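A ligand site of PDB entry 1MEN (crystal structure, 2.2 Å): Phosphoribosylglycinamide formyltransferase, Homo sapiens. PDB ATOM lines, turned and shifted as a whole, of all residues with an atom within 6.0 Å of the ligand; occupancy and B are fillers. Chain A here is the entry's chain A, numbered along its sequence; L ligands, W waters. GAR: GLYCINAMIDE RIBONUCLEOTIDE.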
ATOM      1  N   ILE A  18      32.704 -15.441   2.651  1.00  0.00           N
ATOM      2  CA  ILE A  18      32.306 -14.829   3.915  1.00  0.00           C
ATOM      3  C   ILE A  18      33.365 -15.072   4.978  1.00  0.00           C
ATOM      4  O   ILE A  18      34.267 -15.886   4.776  1.00  0.00           O
ATOM      5  CB  ILE A  18      30.986 -15.431   4.407  1.00  0.00           C
ATOM      6  CG1 ILE A  18      31.170 -16.943   4.647  1.00  0.00           C
ATOM      7  CG2 ILE A  18      29.880 -15.210   3.384  1.00  0.00           C
ATOM      8  CD1 ILE A  18      29.981 -17.611   5.312  1.00  0.00           C
ATOM      9  N   SER A  19      33.246 -14.353   6.098  1.00  0.00           N
ATOM     10  CA  SER A  19      34.155 -14.518   7.241  1.00  0.00           C
ATOM     11  C   SER A  19      33.315 -14.561   8.533  1.00  0.00           C
ATOM     12  O   SER A  19      33.832 -14.896   9.600  1.00  0.00           O
ATOM     13  CB  SER A  19      35.155 -13.346   7.358  1.00  0.00           C
ATOM     14  OG  SER A  19      36.086 -13.283   6.280  1.00  0.00           O
ATOM     15  N   GLY A  20      32.038 -14.217   8.460  1.00  0.00           N
ATOM     16  CA  GLY A  20      31.271 -14.226   9.694  1.00  0.00           C
ATOM     17  C   GLY A  20      29.789 -14.552   9.657  1.00  0.00           C
ATOM     18  O   GLY A  20      29.378 -15.581   9.117  1.00  0.00           O
ATOM     19  N   THR A  21      28.999 -13.646  10.228  1.00  0.00           N
ATOM     20  CA  THR A  21      27.543 -13.785  10.332  1.00  0.00           C
ATOM     21  C   THR A  21      26.759 -14.216   9.089  1.00  0.00           C
ATOM     22  O   THR A  21      25.962 -15.147   9.158  1.00  0.00           O
ATOM     23  CB  THR A  21      26.926 -12.494  10.911  1.00  0.00           C
ATOM     24  OG1 THR A  21      27.386 -12.306  12.256  1.00  0.00           O
ATOM     25  CG2 THR A  21      25.395 -12.603  10.935  1.00  0.00           C
ATOM     26  N   GLY A  22      26.953 -13.533   7.979  1.00  0.00           N
ATOM     27  CA  GLY A  22      26.255 -13.938   6.766  1.00  0.00           C
ATOM     28  C   GLY A  22      24.908 -13.306   6.432  1.00  0.00           C
ATOM     29  O   GLY A  22      24.165 -13.813   5.587  1.00  0.00           O
ATOM     30  N   SER A  23      24.600 -12.177   7.068  1.00  0.00           N
ATOM     31  CA  SER A  23      23.334 -11.521   6.777  1.00  0.00           C
ATOM     32  C   SER A  23      23.294 -11.159   5.306  1.00  0.00           C
ATOM     33  O   SER A  23      22.272 -11.339   4.642  1.00  0.00           O
ATOM     34  CB  SER A  23      23.150 -10.273   7.645  1.00  0.00           C
ATOM     35  OG  SER A  23      24.077  -9.258   7.317  1.00  0.00           O
ATOM     36  N   ASN A  24      24.419 -10.668   4.770  1.00  0.00           N
ATOM     37  CA  ASN A  24      24.458 -10.299   3.353  1.00  0.00           C
ATOM     38  C   ASN A  24      24.326 -11.561   2.497  1.00  0.00           C
ATOM     39  O   ASN A  24      23.671 -11.547   1.451  1.00  0.00           O
ATOM     40  CB  ASN A  24      25.764  -9.549   3.028  1.00  0.00           C
ATOM     41  CG  ASN A  24      25.666  -8.044   3.295  1.00  0.00           C
ATOM     42  OD1 ASN A  24      25.087  -7.300   2.522  1.00  0.00           O
ATOM     43  ND2 ASN A  24      26.255  -7.597   4.409  1.00  0.00           N
ATOM     44  N   LEU A  25      24.961 -12.638   2.938  1.00  0.00           N
ATOM     45  CA  LEU A  25      24.874 -13.915   2.235  1.00  0.00           C
ATOM     46  C   LEU A  25      23.396 -14.315   2.175  1.00  0.00           C
ATOM     47  O   LEU A  25      22.880 -14.717   1.127  1.00  0.00           O
ATOM     48  CB  LEU A  25      25.637 -15.029   2.975  1.00  0.00           C
ATOM     49  CG  LEU A  25      25.194 -16.453   2.588  1.00  0.00           C
ATOM     50  CD1 LEU A  25      25.459 -16.692   1.102  1.00  0.00           C
ATOM     51  CD2 LEU A  25      25.917 -17.504   3.442  1.00  0.00           C
ATOM     52  N   ALA A  97      31.086 -11.119   0.679  1.00  0.00           N
ATOM     53  CA  ALA A  97      30.074 -10.656   1.651  1.00  0.00           C
ATOM     54  C   ALA A  97      30.516 -10.823   3.099  1.00  0.00           C
ATOM     55  O   ALA A  97      30.175 -11.796   3.779  1.00  0.00           O
ATOM     56  CB  ALA A  97      28.758 -11.388   1.401  1.00  0.00           C
ATOM     57  N   GLY A  98      31.285  -9.853   3.567  1.00  0.00           N
ATOM     58  CA  GLY A  98      31.798  -9.896   4.921  1.00  0.00           C
ATOM     59  C   GLY A  98      33.153 -10.599   4.942  1.00  0.00           C
ATOM     60  O   GLY A  98      33.675 -10.921   6.013  1.00  0.00           O
ATOM     61  N   PHE A  99      33.711 -10.831   3.750  1.00  0.00           N
ATOM     62  CA  PHE A  99      35.010 -11.473   3.611  1.00  0.00           C
ATOM     63  C   PHE A  99      36.069 -10.465   4.076  1.00  0.00           C
ATOM     64  O   PHE A  99      36.243  -9.409   3.463  1.00  0.00           O
ATOM     65  CB  PHE A  99      35.249 -11.859   2.151  1.00  0.00           C
ATOM     66  CG  PHE A  99      36.434 -12.748   1.937  1.00  0.00           C
ATOM     67  CD1 PHE A  99      36.554 -13.953   2.634  1.00  0.00           C
ATOM     68  CD2 PHE A  99      37.419 -12.412   1.013  1.00  0.00           C
ATOM     69  CE1 PHE A  99      37.646 -14.818   2.417  1.00  0.00           C
ATOM     70  CE2 PHE A  99      38.513 -13.265   0.776  1.00  0.00           C
ATOM     71  CZ  PHE A  99      38.628 -14.471   1.485  1.00  0.00           C
ATOM     72  N   MET A 100      36.752 -10.781   5.165  1.00  0.00           N
ATOM     73  CA  MET A 100      37.755  -9.876   5.710  1.00  0.00           C
ATOM     74  C   MET A 100      39.192 -10.166   5.279  1.00  0.00           C
ATOM     75  O   MET A 100      40.112 -10.076   6.075  1.00  0.00           O
ATOM     76  CB  MET A 100      37.650  -9.868   7.239  1.00  0.00           C
ATOM     77  CG  MET A 100      36.240  -9.594   7.740  1.00  0.00           C
ATOM     78  SD  MET A 100      35.519  -8.118   6.977  1.00  0.00           S
ATOM     79  CE  MET A 100      35.838  -6.882   8.256  1.00  0.00           C
ATOM     80  N   ASN A 117      32.136  -6.547  -4.126  1.00  0.00           N
ATOM     81  CA  ASN A 117      32.363  -6.477  -2.689  1.00  0.00           C
ATOM     82  C   ASN A 117      31.365  -5.492  -2.145  1.00  0.00           C
ATOM     83  O   ASN A 117      30.939  -4.598  -2.862  1.00  0.00           O
ATOM     84  CB  ASN A 117      33.777  -5.964  -2.404  1.00  0.00           C
ATOM     85  CG  ASN A 117      34.021  -5.770  -0.929  1.00  0.00           C
ATOM     86  OD1 ASN A 117      34.131  -6.732  -0.176  1.00  0.00           O
ATOM     87  ND2 ASN A 117      34.073  -4.504  -0.494  1.00  0.00           N
ATOM     88  N   ILE A 118      30.947  -5.677  -0.894  1.00  0.00           N
ATOM     89  CA  ILE A 118      30.036  -4.738  -0.260  1.00  0.00           C
ATOM     90  C   ILE A 118      30.852  -4.078   0.855  1.00  0.00           C
ATOM     91  O   ILE A 118      31.596  -4.752   1.557  1.00  0.00           O
ATOM     92  CB  ILE A 118      28.785  -5.455   0.306  1.00  0.00           C
ATOM     93  CG1 ILE A 118      27.938  -4.465   1.110  1.00  0.00           C
ATOM     94  CG2 ILE A 118      29.198  -6.659   1.180  1.00  0.00           C
ATOM     95  CD1 ILE A 118      26.845  -3.822   0.312  1.00  0.00           C
ATOM     96  N   HIS A 119      30.763  -2.759   0.981  1.00  0.00           N
ATOM     97  CA  HIS A 119      31.501  -2.045   2.026  1.00  0.00           C
ATOM     98  C   HIS A 119      30.486  -1.177   2.756  1.00  0.00           C
ATOM     99  O   HIS A 119      29.645  -0.548   2.133  1.00  0.00           O
ATOM    100  CB  HIS A 119      32.617  -1.177   1.433  1.00  0.00           C
ATOM    101  CG  HIS A 119      33.561  -0.640   2.461  1.00  0.00           C
ATOM    102  ND1 HIS A 119      34.488  -1.436   3.098  1.00  0.00           N
ATOM    103  CD2 HIS A 119      33.678   0.592   3.002  1.00  0.00           C
ATOM    104  CE1 HIS A 119      35.143  -0.707   3.990  1.00  0.00           C
ATOM    105  NE2 HIS A 119      34.678   0.525   3.948  1.00  0.00           N
ATOM    106  N   PRO A 120      30.577  -1.123   4.084  1.00  0.00           N
ATOM    107  CA  PRO A 120      29.647  -0.331   4.900  1.00  0.00           C
ATOM    108  C   PRO A 120      29.889   1.148   5.061  1.00  0.00           C
ATOM    109  O   PRO A 120      29.853   1.659   6.173  1.00  0.00           O
ATOM    110  CB  PRO A 120      29.663  -1.068   6.247  1.00  0.00           C
ATOM    111  CG  PRO A 120      31.090  -1.480   6.364  1.00  0.00           C
ATOM    112  CD  PRO A 120      31.417  -1.987   4.946  1.00  0.00           C
ATOM    113  N   GLY A 128      38.552   0.591   4.616  1.00  0.00           N
ATOM    114  CA  GLY A 128      39.077  -0.305   5.633  1.00  0.00           C
ATOM    115  C   GLY A 128      38.040  -0.881   6.584  1.00  0.00           C
ATOM    116  O   GLY A 128      36.838  -0.741   6.393  1.00  0.00           O
ATOM    117  N   SER A 129      38.543  -1.546   7.605  1.00  0.00           N
ATOM    118  CA  SER A 129      37.689  -2.177   8.590  1.00  0.00           C
ATOM    119  C   SER A 129      37.155  -1.123   9.541  1.00  0.00           C
ATOM    120  O   SER A 129      37.714  -0.029   9.666  1.00  0.00           O
ATOM    121  CB  SER A 129      38.487  -3.211   9.385  1.00  0.00           C
ATOM    122  OG  SER A 129      39.531  -2.547  10.101  1.00  0.00           O
ATOM    123  N   ASN A 130      36.063  -1.461  10.216  1.00  0.00           N
ATOM    124  CA  ASN A 130      35.429  -0.586  11.189  1.00  0.00           C
ATOM    125  C   ASN A 130      34.978   0.772  10.633  1.00  0.00           C
ATOM    126  O   ASN A 130      35.212   1.818  11.235  1.00  0.00           O
ATOM    127  CB  ASN A 130      36.357  -0.408  12.381  1.00  0.00           C
ATOM    128  CG  ASN A 130      36.692  -1.736  13.086  1.00  0.00           C
ATOM    129  OD1 ASN A 130      37.521  -1.775  13.991  1.00  0.00           O
ATOM    130  ND2 ASN A 130      36.028  -2.825  12.683  1.00  0.00           N
ATOM    131  N   ALA A 131      34.311   0.736   9.477  1.00  0.00           N
ATOM    132  CA  ALA A 131      33.793   1.949   8.861  1.00  0.00           C
ATOM    133  C   ALA A 131      32.810   2.654   9.806  1.00  0.00           C
ATOM    134  O   ALA A 131      32.873   3.869   9.986  1.00  0.00           O
ATOM    135  CB  ALA A 131      33.113   1.606   7.548  1.00  0.00           C
ATOM    136  N   HIS A 132      31.908   1.895  10.420  1.00  0.00           N
ATOM    137  CA  HIS A 132      30.922   2.483  11.334  1.00  0.00           C
ATOM    138  C   HIS A 132      31.589   3.250  12.464  1.00  0.00           C
ATOM    139  O   HIS A 132      31.165   4.360  12.814  1.00  0.00           O
ATOM    140  CB  HIS A 132      30.041   1.394  11.939  1.00  0.00           C
ATOM    141  CG  HIS A 132      29.281   0.597  10.937  1.00  0.00           C
ATOM    142  ND1 HIS A 132      28.297   1.142  10.155  1.00  0.00           N
ATOM    143  CD2 HIS A 132      29.385  -0.707  10.574  1.00  0.00           C
ATOM    144  CE1 HIS A 132      27.802   0.215   9.356  1.00  0.00           C
ATOM    145  NE2 HIS A 132      28.441  -0.916   9.594  1.00  0.00           N
ATOM    146  N   CYS A 145      26.253   2.485   2.401  1.00  0.00           N
ATOM    147  CA  CYS A 145      27.001   1.311   1.995  1.00  0.00           C
ATOM    148  C   CYS A 145      27.288   1.406   0.505  1.00  0.00           C
ATOM    149  O   CYS A 145      26.627   2.167  -0.207  1.00  0.00           O
ATOM    150  CB  CYS A 145      26.190   0.041   2.322  1.00  0.00           C
ATOM    151  SG  CYS A 145      24.506   0.078   1.653  1.00  0.00           S
ATOM    152  N   SER A 177      25.266   0.292  12.656  1.00  0.00           N
ATOM    153  CA  SER A 177      25.642  -0.928  11.959  1.00  0.00           C
ATOM    154  C   SER A 177      24.384  -1.673  11.478  1.00  0.00           C
ATOM    155  O   SER A 177      24.306  -2.146  10.341  1.00  0.00           O
ATOM    156  CB  SER A 177      26.459  -1.800  12.911  1.00  0.00           C
ATOM    157  OG  SER A 177      26.873  -3.000  12.308  1.00  0.00           O
ATOM    158  N   VAL A 180      22.657   0.250   8.680  1.00  0.00           N
ATOM    159  CA  VAL A 180      23.391   0.154   7.420  1.00  0.00           C
ATOM    160  C   VAL A 180      23.230  -1.204   6.747  1.00  0.00           C
ATOM    161  O   VAL A 180      23.164  -1.293   5.501  1.00  0.00           O
ATOM    162  CB  VAL A 180      24.917   0.418   7.582  1.00  0.00           C
ATOM    163  CG1 VAL A 180      25.645   0.153   6.253  1.00  0.00           C
ATOM    164  CG2 VAL A 180      25.149   1.871   8.011  1.00  0.00           C
ATOM    165  N   LYS A 181      23.177  -2.269   7.545  1.00  0.00           N
ATOM    166  CA  LYS A 181      23.023  -3.594   6.971  1.00  0.00           C
ATOM    167  C   LYS A 181      21.705  -3.719   6.189  1.00  0.00           C
ATOM    168  O   LYS A 181      21.652  -4.392   5.160  1.00  0.00           O
ATOM    169  CB  LYS A 181      23.100  -4.689   8.038  1.00  0.00           C
ATOM    170  CG  LYS A 181      24.535  -5.109   8.364  1.00  0.00           C
ATOM    171  CD  LYS A 181      24.595  -6.373   9.220  1.00  0.00           C
ATOM    172  CE  LYS A 181      26.040  -6.829   9.461  1.00  0.00           C
ATOM    173  NZ  LYS A 181      26.101  -8.091  10.280  1.00  0.00           N
ATOM    174  N   GLU A 184      22.410  -2.528   2.848  1.00  0.00           N
ATOM    175  CA  GLU A 184      23.290  -3.483   2.177  1.00  0.00           C
ATOM    176  C   GLU A 184      22.519  -4.639   1.532  1.00  0.00           C
ATOM    177  O   GLU A 184      22.813  -5.066   0.409  1.00  0.00           O
ATOM    178  CB  GLU A 184      24.273  -4.096   3.172  1.00  0.00           C
ATOM    179  CG  GLU A 184      25.329  -3.177   3.755  1.00  0.00           C
ATOM    180  CD  GLU A 184      26.254  -3.924   4.719  1.00  0.00           C
ATOM    181  OE1 GLU A 184      26.797  -4.973   4.316  1.00  0.00           O
ATOM    182  OE2 GLU A 184      26.447  -3.465   5.876  1.00  0.00           O
ATOM    183  N   HIS A 185      21.533  -5.143   2.267  1.00  0.00           N
ATOM    184  CA  HIS A 185      20.724  -6.250   1.781  1.00  0.00           C
ATOM    185  C   HIS A 185      19.906  -5.807   0.585  1.00  0.00           C
ATOM    186  O   HIS A 185      19.469  -6.623  -0.215  1.00  0.00           O
ATOM    187  CB  HIS A 185      19.827  -6.790   2.898  1.00  0.00           C
ATOM    188  CG  HIS A 185      20.594  -7.225   4.113  1.00  0.00           C
ATOM    189  ND1 HIS A 185      20.046  -7.294   5.372  1.00  0.00           N
ATOM    190  CD2 HIS A 185      21.904  -7.578   4.251  1.00  0.00           C
ATOM    191  CE1 HIS A 185      20.978  -7.659   6.240  1.00  0.00           C
ATOM    192  NE2 HIS A 185      22.109  -7.843   5.586  1.00  0.00           N
HETATM  193  C1  GAR L   1      28.780  -6.106   6.508  1.00  0.00           C
HETATM  194  O6  GAR L   1      28.082  -5.016   7.161  1.00  0.00           O
HETATM  195  C2  GAR L   1      29.712  -5.658   5.355  1.00  0.00           C
HETATM  196  O8  GAR L   1      29.252  -4.462   4.714  1.00  0.00           O
HETATM  197  C3  GAR L   1      30.981  -5.388   6.089  1.00  0.00           C
HETATM  198  O4  GAR L   1      31.041  -6.367   7.141  1.00  0.00           O
HETATM  199  C5  GAR L   1      29.701  -6.773   7.503  1.00  0.00           C
HETATM  200  C10 GAR L   1      29.524  -8.318   7.504  1.00  0.00           C
HETATM  201  O12 GAR L   1      28.115  -8.646   7.420  1.00  0.00           O
HETATM  202  N19 GAR L   1      32.187  -5.541   5.330  1.00  0.00           N
HETATM  203  C21 GAR L   1      33.372  -4.977   5.608  1.00  0.00           C
HETATM  204  O22 GAR L   1      33.571  -4.276   6.629  1.00  0.00           O
HETATM  205  C23 GAR L   1      34.473  -5.197   4.570  1.00  0.00           C
HETATM  206  N24 GAR L   1      35.825  -5.643   4.997  1.00  0.00           N
HETATM  207  P15 GAR L   1      27.511 -10.074   7.336  1.00  0.00           P
HETATM  208  O16 GAR L   1      27.008 -10.034   5.840  1.00  0.00           O
HETATM  209  O17 GAR L   1      26.290 -10.196   8.384  1.00  0.00           O
HETATM  210  O18 GAR L   1      28.445 -11.120   7.562  1.00  0.00           O
HETATM  211  O   HOH W   1      27.313 -12.083   4.242  1.00  0.00           O
HETATM  212  O   HOH W   2      35.338  -3.799   1.845  1.00  0.00           O
HETATM  213  O   HOH W   3      30.672 -12.713   6.259  1.00  0.00           O
HETATM  214  O   HOH W   4      29.791 -10.630   9.815  1.00  0.00           O
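The side-chain carboxylate (OE1) of Glu 184 lies within hydrogen-bond range of an oxygen (O8) of the ligand (2.5 Å). The backbone NH (N) of Ser 23 sits at hydrogen-bond distance from an oxygen (O17) of the ligand, 2.9 Å away. The side-chain hydroxyl (OG) of Ser 23 lies within hydrogen-bond range of an oxygen (O17) of the ligand, 2.6 Å away. The side-chain amino group of Lys 181 lies within salt-bridge range of an oxygen (O17) of the ligand, at 2.8 Å. The backbone NH of Gly 22 is in hydrogen-bond range of an oxygen (O18) of the ligand, at 2.9 Å. N of Asn 24 is in hydrogen-bond range of O16 of the ligand, 2.9 Å away. An oxygen (O16) of the ligand lies within hydrogen-bond range of the side-chain amide nitrogen (ND2) of Asn 24 (2.9 Å). The side-chain sulfur (SD) of Met 100 is in hydrogen-bond range of a nitrogen (N24) of the ligand (3.2 Å).
The side-chain carboxylate of Glu 184 sits at hydrogen-bond distance from the side-chain amide nitrogen of Asn 24 (2.7 Å). The backbone NH (N) of Glu 184 is in hydrogen-bond range of the side-chain sulfur (SG) of Cys 145, at 3.6 Å. The side-chain hydroxyl (OG) of Ser 23 is in hydrogen-bond range of a ring nitrogen (NE2) of His 185, at 3.0 Å. The backbone carbonyl oxygen (O) of Lys 181 lies close to a ring nitrogen (ND1) of His 185. The side-chain hydroxyl of Ser 19 is in hydrogen-bond range of the backbone NH of Met 100, 2.8 Å away. The backbone carbonyl oxygen (O) of Gly 98 sits close to the side-chain hydroxyl (OG) of Ser 19 (3.4 Å).
Thr 21 touches the ligand. Gly 98 touches the ligand (CA to C10, 3.8 Å). Ile 118 touches the ligand (CG1 to O8, 3.8 Å). Pro 120 touches the ligand (CD to O8, 3.3 Å). Hydrophobic or aromatic side chains that line the ligand: Met 100, Ile 118 and Pro 120. Ten residues have an atom within 4 Å of the ligand: Thr 21, Gly 22, Ser 23, Asn 24, Gly 98, Met 100, Ile 118, Pro 120, Lys 181 and Glu 184.
Water W1 lies within hydrogen-bond range of O16 of the ligand, N of Leu 25, O of Ala 97 and N of Asn 24. Water W4 bridges an oxygen (O18) of the ligand (2.7 Å) and the backbone NH of Thr 21 (3.1 Å). Water W3 lies within hydrogen-bond range of O of Ala 97 (2.7 Å), N of Gly 20 (3.0 Å), O18 of the ligand (3.0 Å) and N of Ser 19 (3.1 Å). Water W2 lies within hydrogen-bond range of the side-chain amide nitrogen (ND2) of Asn 117 (2.8 Å) and a ring nitrogen (ND1) of His 119 (2.8 Å).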
